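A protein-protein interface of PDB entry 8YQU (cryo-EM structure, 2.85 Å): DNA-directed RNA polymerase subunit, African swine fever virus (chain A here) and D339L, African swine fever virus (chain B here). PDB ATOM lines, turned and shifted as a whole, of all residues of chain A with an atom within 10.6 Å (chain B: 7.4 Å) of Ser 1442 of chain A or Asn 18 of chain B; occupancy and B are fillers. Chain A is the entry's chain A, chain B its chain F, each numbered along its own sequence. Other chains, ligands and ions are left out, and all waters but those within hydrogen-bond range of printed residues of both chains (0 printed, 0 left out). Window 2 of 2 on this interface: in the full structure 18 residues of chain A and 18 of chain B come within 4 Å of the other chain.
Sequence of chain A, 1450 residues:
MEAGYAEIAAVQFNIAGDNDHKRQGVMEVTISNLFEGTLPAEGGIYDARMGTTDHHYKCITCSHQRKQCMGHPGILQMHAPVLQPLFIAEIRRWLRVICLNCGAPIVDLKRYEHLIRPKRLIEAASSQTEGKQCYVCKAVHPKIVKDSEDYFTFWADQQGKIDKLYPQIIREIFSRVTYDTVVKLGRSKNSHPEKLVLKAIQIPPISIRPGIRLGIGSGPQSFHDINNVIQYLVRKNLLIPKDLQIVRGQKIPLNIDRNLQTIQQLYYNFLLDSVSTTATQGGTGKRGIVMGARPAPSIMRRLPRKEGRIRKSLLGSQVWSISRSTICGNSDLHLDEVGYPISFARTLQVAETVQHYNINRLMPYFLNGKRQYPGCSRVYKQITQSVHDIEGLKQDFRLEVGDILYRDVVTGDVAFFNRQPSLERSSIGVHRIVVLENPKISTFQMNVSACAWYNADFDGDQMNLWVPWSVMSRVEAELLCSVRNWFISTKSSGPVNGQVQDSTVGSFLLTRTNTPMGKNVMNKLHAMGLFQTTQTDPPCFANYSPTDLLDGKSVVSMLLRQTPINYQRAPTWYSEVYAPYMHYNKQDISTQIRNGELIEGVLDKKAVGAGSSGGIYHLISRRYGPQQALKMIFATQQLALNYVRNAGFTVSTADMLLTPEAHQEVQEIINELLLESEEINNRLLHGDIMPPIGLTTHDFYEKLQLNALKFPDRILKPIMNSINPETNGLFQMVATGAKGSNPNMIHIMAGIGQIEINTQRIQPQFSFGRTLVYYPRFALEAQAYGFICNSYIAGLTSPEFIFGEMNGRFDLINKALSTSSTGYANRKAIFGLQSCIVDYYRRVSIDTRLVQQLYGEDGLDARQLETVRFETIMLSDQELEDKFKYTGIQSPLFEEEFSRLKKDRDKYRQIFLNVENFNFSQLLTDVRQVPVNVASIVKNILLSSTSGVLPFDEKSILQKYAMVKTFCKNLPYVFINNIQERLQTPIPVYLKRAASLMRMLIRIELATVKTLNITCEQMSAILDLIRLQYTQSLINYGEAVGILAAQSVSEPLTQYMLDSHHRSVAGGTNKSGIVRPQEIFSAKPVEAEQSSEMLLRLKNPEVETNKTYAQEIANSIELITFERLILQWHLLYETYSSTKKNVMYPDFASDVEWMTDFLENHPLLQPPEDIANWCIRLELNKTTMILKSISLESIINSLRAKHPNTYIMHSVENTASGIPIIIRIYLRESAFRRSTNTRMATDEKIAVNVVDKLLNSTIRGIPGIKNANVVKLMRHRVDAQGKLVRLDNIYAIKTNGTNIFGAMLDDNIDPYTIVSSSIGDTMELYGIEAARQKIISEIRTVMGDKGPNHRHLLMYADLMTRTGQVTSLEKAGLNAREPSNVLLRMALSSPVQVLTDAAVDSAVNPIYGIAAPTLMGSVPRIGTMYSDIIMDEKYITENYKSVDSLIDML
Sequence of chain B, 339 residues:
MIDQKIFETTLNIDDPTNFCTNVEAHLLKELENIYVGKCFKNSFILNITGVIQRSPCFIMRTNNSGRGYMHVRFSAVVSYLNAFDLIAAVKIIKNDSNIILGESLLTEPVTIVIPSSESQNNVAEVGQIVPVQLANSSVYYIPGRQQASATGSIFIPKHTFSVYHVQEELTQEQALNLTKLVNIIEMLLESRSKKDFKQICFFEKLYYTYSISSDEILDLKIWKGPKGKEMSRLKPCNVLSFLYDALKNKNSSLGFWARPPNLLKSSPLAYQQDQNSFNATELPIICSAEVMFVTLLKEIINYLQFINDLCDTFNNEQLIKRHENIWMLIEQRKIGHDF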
ATOM      1  N   MET A1431      22.720  17.145  23.359  1.00  0.00           N
ATOM      2  CA  MET A1431      21.803  16.094  22.949  1.00  0.00           C
ATOM      3  C   MET A1431      21.398  16.293  21.495  1.00  0.00           C
ATOM      4  O   MET A1431      21.062  17.404  21.074  1.00  0.00           O
ATOM      5  CB  MET A1431      20.563  16.097  23.841  1.00  0.00           C
ATOM      6  CG  MET A1431      20.787  15.517  25.228  1.00  0.00           C
ATOM      7  SD  MET A1431      21.518  13.873  25.269  1.00  0.00           S
ATOM      8  CE  MET A1431      20.387  12.958  24.233  1.00  0.00           C
ATOM      9  N   ASP A1432      21.428  15.209  20.724  1.00  0.00           N
ATOM     10  CA  ASP A1432      21.106  15.261  19.298  1.00  0.00           C
ATOM     11  C   ASP A1432      19.593  15.362  19.147  1.00  0.00           C
ATOM     12  O   ASP A1432      18.876  14.360  19.139  1.00  0.00           O
ATOM     13  CB  ASP A1432      21.665  14.044  18.575  1.00  0.00           C
ATOM     14  CG  ASP A1432      21.883  14.296  17.099  1.00  0.00           C
ATOM     15  OD1 ASP A1432      21.427  15.346  16.600  1.00  0.00           O
ATOM     16  OD2 ASP A1432      22.518  13.449  16.440  1.00  0.00           O
ATOM     17  N   GLU A1433      19.105  16.596  19.025  1.00  0.00           N
ATOM     18  CA  GLU A1433      17.665  16.829  18.966  1.00  0.00           C
ATOM     19  C   GLU A1433      17.054  16.237  17.701  1.00  0.00           C
ATOM     20  O   GLU A1433      16.019  15.564  17.757  1.00  0.00           O
ATOM     21  CB  GLU A1433      17.380  18.330  19.051  1.00  0.00           C
ATOM     22  CG  GLU A1433      15.905  18.682  19.111  1.00  0.00           C
ATOM     23  CD  GLU A1433      15.375  19.209  17.794  1.00  0.00           C
ATOM     24  OE1 GLU A1433      16.177  19.745  17.001  1.00  0.00           O
ATOM     25  OE2 GLU A1433      14.156  19.090  17.551  1.00  0.00           O
ATOM     26  N   ILE A1436      16.932  12.200  17.550  1.00  0.00           N
ATOM     27  CA  ILE A1436      16.046  11.516  18.487  1.00  0.00           C
ATOM     28  C   ILE A1436      14.595  11.586  18.023  1.00  0.00           C
ATOM     29  O   ILE A1436      13.851  10.604  18.126  1.00  0.00           O
ATOM     30  CB  ILE A1436      16.218  12.101  19.900  1.00  0.00           C
ATOM     31  CG1 ILE A1436      17.580  11.711  20.470  1.00  0.00           C
ATOM     32  CG2 ILE A1436      15.105  11.632  20.821  1.00  0.00           C
ATOM     33  CD1 ILE A1436      17.915  12.413  21.754  1.00  0.00           C
ATOM     34  N   THR A1437      14.170  12.743  17.506  1.00  0.00           N
ATOM     35  CA  THR A1437      12.761  12.935  17.175  1.00  0.00           C
ATOM     36  C   THR A1437      12.290  11.938  16.123  1.00  0.00           C
ATOM     37  O   THR A1437      11.211  11.350  16.255  1.00  0.00           O
ATOM     38  CB  THR A1437      12.522  14.365  16.690  1.00  0.00           C
ATOM     39  OG1 THR A1437      13.386  14.646  15.583  1.00  0.00           O
ATOM     40  CG2 THR A1437      12.794  15.358  17.806  1.00  0.00           C
ATOM     41  N   GLU A1438      13.085  11.732  15.074  1.00  0.00           N
ATOM     42  CA  GLU A1438      12.691  10.808  14.018  1.00  0.00           C
ATOM     43  C   GLU A1438      12.871   9.356  14.441  1.00  0.00           C
ATOM     44  O   GLU A1438      12.115   8.486  13.993  1.00  0.00           O
ATOM     45  CB  GLU A1438      13.489  11.113  12.744  1.00  0.00           C
ATOM     46  CG  GLU A1438      13.052  10.364  11.478  1.00  0.00           C
ATOM     47  CD  GLU A1438      13.514   8.919  11.433  1.00  0.00           C
ATOM     48  OE1 GLU A1438      14.555   8.605  12.044  1.00  0.00           O
ATOM     49  OE2 GLU A1438      12.833   8.096  10.784  1.00  0.00           O
ATOM     50  N   ASN A1439      13.836   9.077  15.314  1.00  0.00           N
ATOM     51  CA  ASN A1439      14.236   7.710  15.620  1.00  0.00           C
ATOM     52  C   ASN A1439      13.683   7.167  16.929  1.00  0.00           C
ATOM     53  O   ASN A1439      13.388   5.973  17.005  1.00  0.00           O
ATOM     54  CB  ASN A1439      15.765   7.609  15.648  1.00  0.00           C
ATOM     55  CG  ASN A1439      16.363   7.491  14.264  1.00  0.00           C
ATOM     56  OD1 ASN A1439      16.017   6.589  13.502  1.00  0.00           O
ATOM     57  ND2 ASN A1439      17.250   8.413  13.924  1.00  0.00           N
ATOM     58  N   TYR A1440      13.535   7.997  17.955  1.00  0.00           N
ATOM     59  CA  TYR A1440      13.090   7.541  19.264  1.00  0.00           C
ATOM     60  C   TYR A1440      11.630   7.915  19.494  1.00  0.00           C
ATOM     61  O   TYR A1440      11.029   8.685  18.741  1.00  0.00           O
ATOM     62  CB  TYR A1440      13.969   8.121  20.380  1.00  0.00           C
ATOM     63  CG  TYR A1440      15.362   7.533  20.450  1.00  0.00           C
ATOM     64  CD1 TYR A1440      16.255   7.671  19.396  1.00  0.00           C
ATOM     65  CD2 TYR A1440      15.782   6.834  21.574  1.00  0.00           C
ATOM     66  CE1 TYR A1440      17.525   7.134  19.460  1.00  0.00           C
ATOM     67  CE2 TYR A1440      17.051   6.292  21.646  1.00  0.00           C
ATOM     68  CZ  TYR A1440      17.918   6.446  20.587  1.00  0.00           C
ATOM     69  OH  TYR A1440      19.183   5.909  20.653  1.00  0.00           O
ATOM     70  N   LYS A1441      11.065   7.349  20.559  1.00  0.00           N
ATOM     71  CA  LYS A1441       9.669   7.553  20.911  1.00  0.00           C
ATOM     72  C   LYS A1441       9.563   7.948  22.377  1.00  0.00           C
ATOM     73  O   LYS A1441      10.442   7.650  23.189  1.00  0.00           O
ATOM     74  CB  LYS A1441       8.832   6.292  20.650  1.00  0.00           C
ATOM     75  CG  LYS A1441       8.813   5.836  19.201  1.00  0.00           C
ATOM     76  CD  LYS A1441       8.163   6.875  18.302  1.00  0.00           C
ATOM     77  CE  LYS A1441       7.964   6.337  16.894  1.00  0.00           C
ATOM     78  NZ  LYS A1441       9.258   6.124  16.190  1.00  0.00           N
ATOM     79  N   SER A1442       8.469   8.627  22.706  1.00  0.00           N
ATOM     80  CA  SER A1442       8.203   9.035  24.080  1.00  0.00           C
ATOM     81  C   SER A1442       7.542   7.905  24.864  1.00  0.00           C
ATOM     82  O   SER A1442       7.929   7.612  25.995  1.00  0.00           O
ATOM     83  CB  SER A1442       7.317  10.282  24.111  1.00  0.00           C
ATOM     84  OG  SER A1442       7.977  11.393  23.530  1.00  0.00           O
ATOM     85  N   ILE B  13      16.800  18.930  32.969  1.00  0.00           N
ATOM     86  CA  ILE B  13      16.113  17.831  32.303  1.00  0.00           C
ATOM     87  C   ILE B  13      16.658  16.526  32.863  1.00  0.00           C
ATOM     88  O   ILE B  13      17.814  16.167  32.604  1.00  0.00           O
ATOM     89  CB  ILE B  13      16.292  17.887  30.779  1.00  0.00           C
ATOM     90  CG1 ILE B  13      15.636  19.139  30.187  1.00  0.00           C
ATOM     91  CG2 ILE B  13      15.757  16.625  30.153  1.00  0.00           C
ATOM     92  CD1 ILE B  13      16.543  20.348  30.115  1.00  0.00           C
ATOM     93  N   ASP B  15      15.769  13.327  32.220  1.00  0.00           N
ATOM     94  CA  ASP B  15      15.977  12.311  31.190  1.00  0.00           C
ATOM     95  C   ASP B  15      16.044  13.004  29.837  1.00  0.00           C
ATOM     96  O   ASP B  15      15.005  13.277  29.215  1.00  0.00           O
ATOM     97  CB  ASP B  15      14.870  11.261  31.218  1.00  0.00           C
ATOM     98  CG  ASP B  15      15.187  10.065  30.346  1.00  0.00           C
ATOM     99  OD1 ASP B  15      16.013   9.229  30.765  1.00  0.00           O
ATOM    100  OD2 ASP B  15      14.617   9.963  29.242  1.00  0.00           O
ATOM    101  N   PRO B  16      17.245  13.319  29.348  1.00  0.00           N
ATOM    102  CA  PRO B  16      17.352  14.033  28.065  1.00  0.00           C
ATOM    103  C   PRO B  16      16.769  13.277  26.884  1.00  0.00           C
ATOM    104  O   PRO B  16      16.239  13.909  25.961  1.00  0.00           O
ATOM    105  CB  PRO B  16      18.866  14.238  27.911  1.00  0.00           C
ATOM    106  CG  PRO B  16      19.414  14.114  29.297  1.00  0.00           C
ATOM    107  CD  PRO B  16      18.562  13.085  29.960  1.00  0.00           C
ATOM    108  N   THR B  17      16.849  11.945  26.881  1.00  0.00           N
ATOM    109  CA  THR B  17      16.399  11.175  25.724  1.00  0.00           C
ATOM    110  C   THR B  17      14.899  11.331  25.504  1.00  0.00           C
ATOM    111  O   THR B  17      14.450  11.618  24.388  1.00  0.00           O
ATOM    112  CB  THR B  17      16.766   9.701  25.900  1.00  0.00           C
ATOM    113  OG1 THR B  17      18.124   9.596  26.346  1.00  0.00           O
ATOM    114  CG2 THR B  17      16.613   8.956  24.584  1.00  0.00           C
ATOM    115  N   ASN B  18      14.104  11.140  26.559  1.00  0.00           N
ATOM    116  CA  ASN B  18      12.661  11.324  26.442  1.00  0.00           C
ATOM    117  C   ASN B  18      12.312  12.782  26.171  1.00  0.00           C
ATOM    118  O   ASN B  18      11.383  13.075  25.409  1.00  0.00           O
ATOM    119  CB  ASN B  18      11.967  10.833  27.712  1.00  0.00           C
ATOM    120  CG  ASN B  18      10.457  10.816  27.586  1.00  0.00           C
ATOM    121  OD1 ASN B  18       9.911  10.929  26.490  1.00  0.00           O
ATOM    122  ND2 ASN B  18       9.773  10.676  28.715  1.00  0.00           N
ATOM    123  N   PHE B  19      13.045  13.708  26.792  1.00  0.00           N
ATOM    124  CA  PHE B  19      12.761  15.129  26.630  1.00  0.00           C
ATOM    125  C   PHE B  19      12.943  15.574  25.185  1.00  0.00           C
ATOM    126  O   PHE B  19      12.134  16.348  24.659  1.00  0.00           O
ATOM    127  CB  PHE B  19      13.668  15.936  27.555  1.00  0.00           C
ATOM    128  CG  PHE B  19      13.431  17.418  27.515  1.00  0.00           C
ATOM    129  CD1 PHE B  19      12.460  17.999  28.311  1.00  0.00           C
ATOM    130  CD2 PHE B  19      14.190  18.234  26.693  1.00  0.00           C
ATOM    131  CE1 PHE B  19      12.245  19.363  28.282  1.00  0.00           C
ATOM    132  CE2 PHE B  19      13.977  19.597  26.659  1.00  0.00           C
ATOM    133  CZ  PHE B  19      13.004  20.161  27.454  1.00  0.00           C
ATOM    134  N   CYS B  20      13.999  15.097  24.526  1.00  0.00           N
ATOM    135  CA  CYS B  20      14.302  15.549  23.175  1.00  0.00           C
ATOM    136  C   CYS B  20      13.339  15.005  22.128  1.00  0.00           C
ATOM    137  O   CYS B  20      13.393  15.452  20.978  1.00  0.00           O
ATOM    138  CB  CYS B  20      15.736  15.172  22.804  1.00  0.00           C
ATOM    139  SG  CYS B  20      16.995  16.094  23.711  1.00  0.00           S
ATOM    140  N   THR B  21      12.471  14.056  22.488  1.00  0.00           N
ATOM    141  CA  THR B  21      11.515  13.530  21.517  1.00  0.00           C
ATOM    142  C   THR B  21      10.536  14.606  21.064  1.00  0.00           C
ATOM    143  O   THR B  21      10.255  14.733  19.866  1.00  0.00           O
ATOM    144  CB  THR B  21      10.767  12.337  22.110  1.00  0.00           C
ATOM    145  OG1 THR B  21      10.016  12.762  23.254  1.00  0.00           O
ATOM    146  CG2 THR B  21      11.744  11.251  22.528  1.00  0.00           C
ATOM    147  N   ASN B  22      10.002  15.389  22.003  1.00  0.00           N
ATOM    148  CA  ASN B  22       9.140  16.531  21.691  1.00  0.00           C
ATOM    149  C   ASN B  22       9.628  17.701  22.540  1.00  0.00           C
ATOM    150  O   ASN B  22       9.102  17.959  23.629  1.00  0.00           O
ATOM    151  CB  ASN B  22       7.674  16.205  21.950  1.00  0.00           C
ATOM    152  CG  ASN B  22       6.734  17.057  21.124  1.00  0.00           C
ATOM    153  OD1 ASN B  22       7.164  17.969  20.418  1.00  0.00           O
ATOM    154  ND2 ASN B  22       5.443  16.758  21.199  1.00  0.00           N
ATOM    155  N   VAL B  23      10.623  18.420  22.014  1.00  0.00           N
ATOM    156  CA  VAL B  23      11.314  19.438  22.798  1.00  0.00           C
ATOM    157  C   VAL B  23      10.374  20.585  23.137  1.00  0.00           C
ATOM    158  O   VAL B  23      10.309  21.030  24.286  1.00  0.00           O
ATOM    159  CB  VAL B  23      12.561  19.940  22.050  1.00  0.00           C
ATOM    160  CG1 VAL B  23      13.240  21.045  22.840  1.00  0.00           C
ATOM    161  CG2 VAL B  23      13.521  18.796  21.801  1.00  0.00           C
ATOM    162  N   HIS B  26       7.561  19.455  25.673  1.00  0.00           N
ATOM    163  CA  HIS B  26       8.102  19.234  27.010  1.00  0.00           C
ATOM    164  C   HIS B  26       8.547  20.545  27.648  1.00  0.00           C
ATOM    165  O   HIS B  26       8.355  20.752  28.852  1.00  0.00           O
ATOM    166  CB  HIS B  26       9.259  18.239  26.950  1.00  0.00           C
ATOM    167  CG  HIS B  26       8.837  16.839  26.628  1.00  0.00           C
ATOM    168  ND1 HIS B  26       8.806  16.347  25.342  1.00  0.00           N
ATOM    169  CD2 HIS B  26       8.432  15.826  27.428  1.00  0.00           C
ATOM    170  CE1 HIS B  26       8.399  15.092  25.362  1.00  0.00           C
ATOM    171  NE2 HIS B  26       8.165  14.750  26.616  1.00  0.00           N
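Hydrophobic or aromatic side chains of chain B within 4 Å of the printed part of chain A: Pro 16 and Val 23.
Of the 10 printed residues of chain A, 7 touch a printed residue of chain B.
Printed residues of chain A that touch a printed residue of chain B: Met 1431, Glu 1433, Ile 1436, Thr 1437, Tyr 1440, Lys 1441 and Ser 1442.
Among the printed residues, 12 pairs touch across the chains.
Among the printed residues, no Asp or Glu carboxylate lies within 4 Å of a Lys or Arg side-chain nitrogen of the other chain.
Of the printed residues of chain B, Glu 1433 of chain A touches Val 23 (3.6 Å).
Printed residues of chain B within 4 Å of Thr 1437 of chain A: Cys 20 and Thr 21.
Of the printed residues of chain B, Tyr 1440 of chain A touches Thr 17.
Of the printed residues of chain B, Lys 1441 of chain A touches Thr 21.
Of chain B, only Asn 18 and Thr 21 come within 4 Å of Ser 1442 of chain A.
Asp 15 of chain B touches none of the printed residues of chain A.
Of chain A, only Ser 1442 comes within 4 Å of Asn 18 of chain B.
Cys 20 of chain B touches just these residues of chain A: Met 1431 (3.6 Å), Ile 1436 (3.7 Å) and Thr 1437 (3.2 Å).
Of chain A, only Ile 1436 (3.8 Å), Thr 1437 (3.3 Å), Lys 1441 (3.9 Å) and Ser 1442 (2.5 Å) come within 4 Å of Thr 21 of chain B.
The nearest residue of chain A that does not touch Asn 18 of chain B is Lys 1441 of chain A (4.7 Å).
The nearest printed residue of chain B that does not touch Thr 1437 of chain A is Asn 22 of chain B (5.0 Å).
The side-chain hydroxyl of Ser 1442 of chain A is in hydrogen-bond range of the side-chain hydroxyl of Thr 21 of chain B (2.5 Å).
O of Pro 16 of chain B is in hydrogen-bond range of SG of Cys 20 of chain B (3.2 Å).
N of Asn 18 of chain B sits at hydrogen-bond distance from OD2 of Asp 15 of chain B (3.0 Å).
O of Asn 18 of chain B sits at hydrogen-bond distance from OG1 of Thr 21 of chain B, at 2.6 Å.
Pro 16 of chain B touches Met 1431 of chain A (CB to CG, 3.5 Å).
Cys 20 of chain B touches Met 1431 of chain A (SG to CB, 3.6 Å).
Val 23 of chain B touches Glu 1433 of chain A (CG2 to CG, 3.6 Å).
Ile 1436 of chain A touches Thr 17 of chain B (CG2 to O, 3.6 Å).
Cys 20 of chain B touches Ile 1436 of chain A.
Thr 1437 of chain A touches Cys 20 of chain B (CG2 to O, 3.2 Å).
CG2 of Thr 1437 of chain A touches O of Thr 21 of chain B, at 3.3 Å.
CG2 of Thr 17 of chain B touches CD2 of Tyr 1440 of chain A, at 3.8 Å.
O of Lys 1441 of chain A touches CG2 of Thr 21 of chain B, at 3.9 Å.
CA of Ser 1442 of chain A touches OD1 of Asn 18 of chain B, 3.5 Å away.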
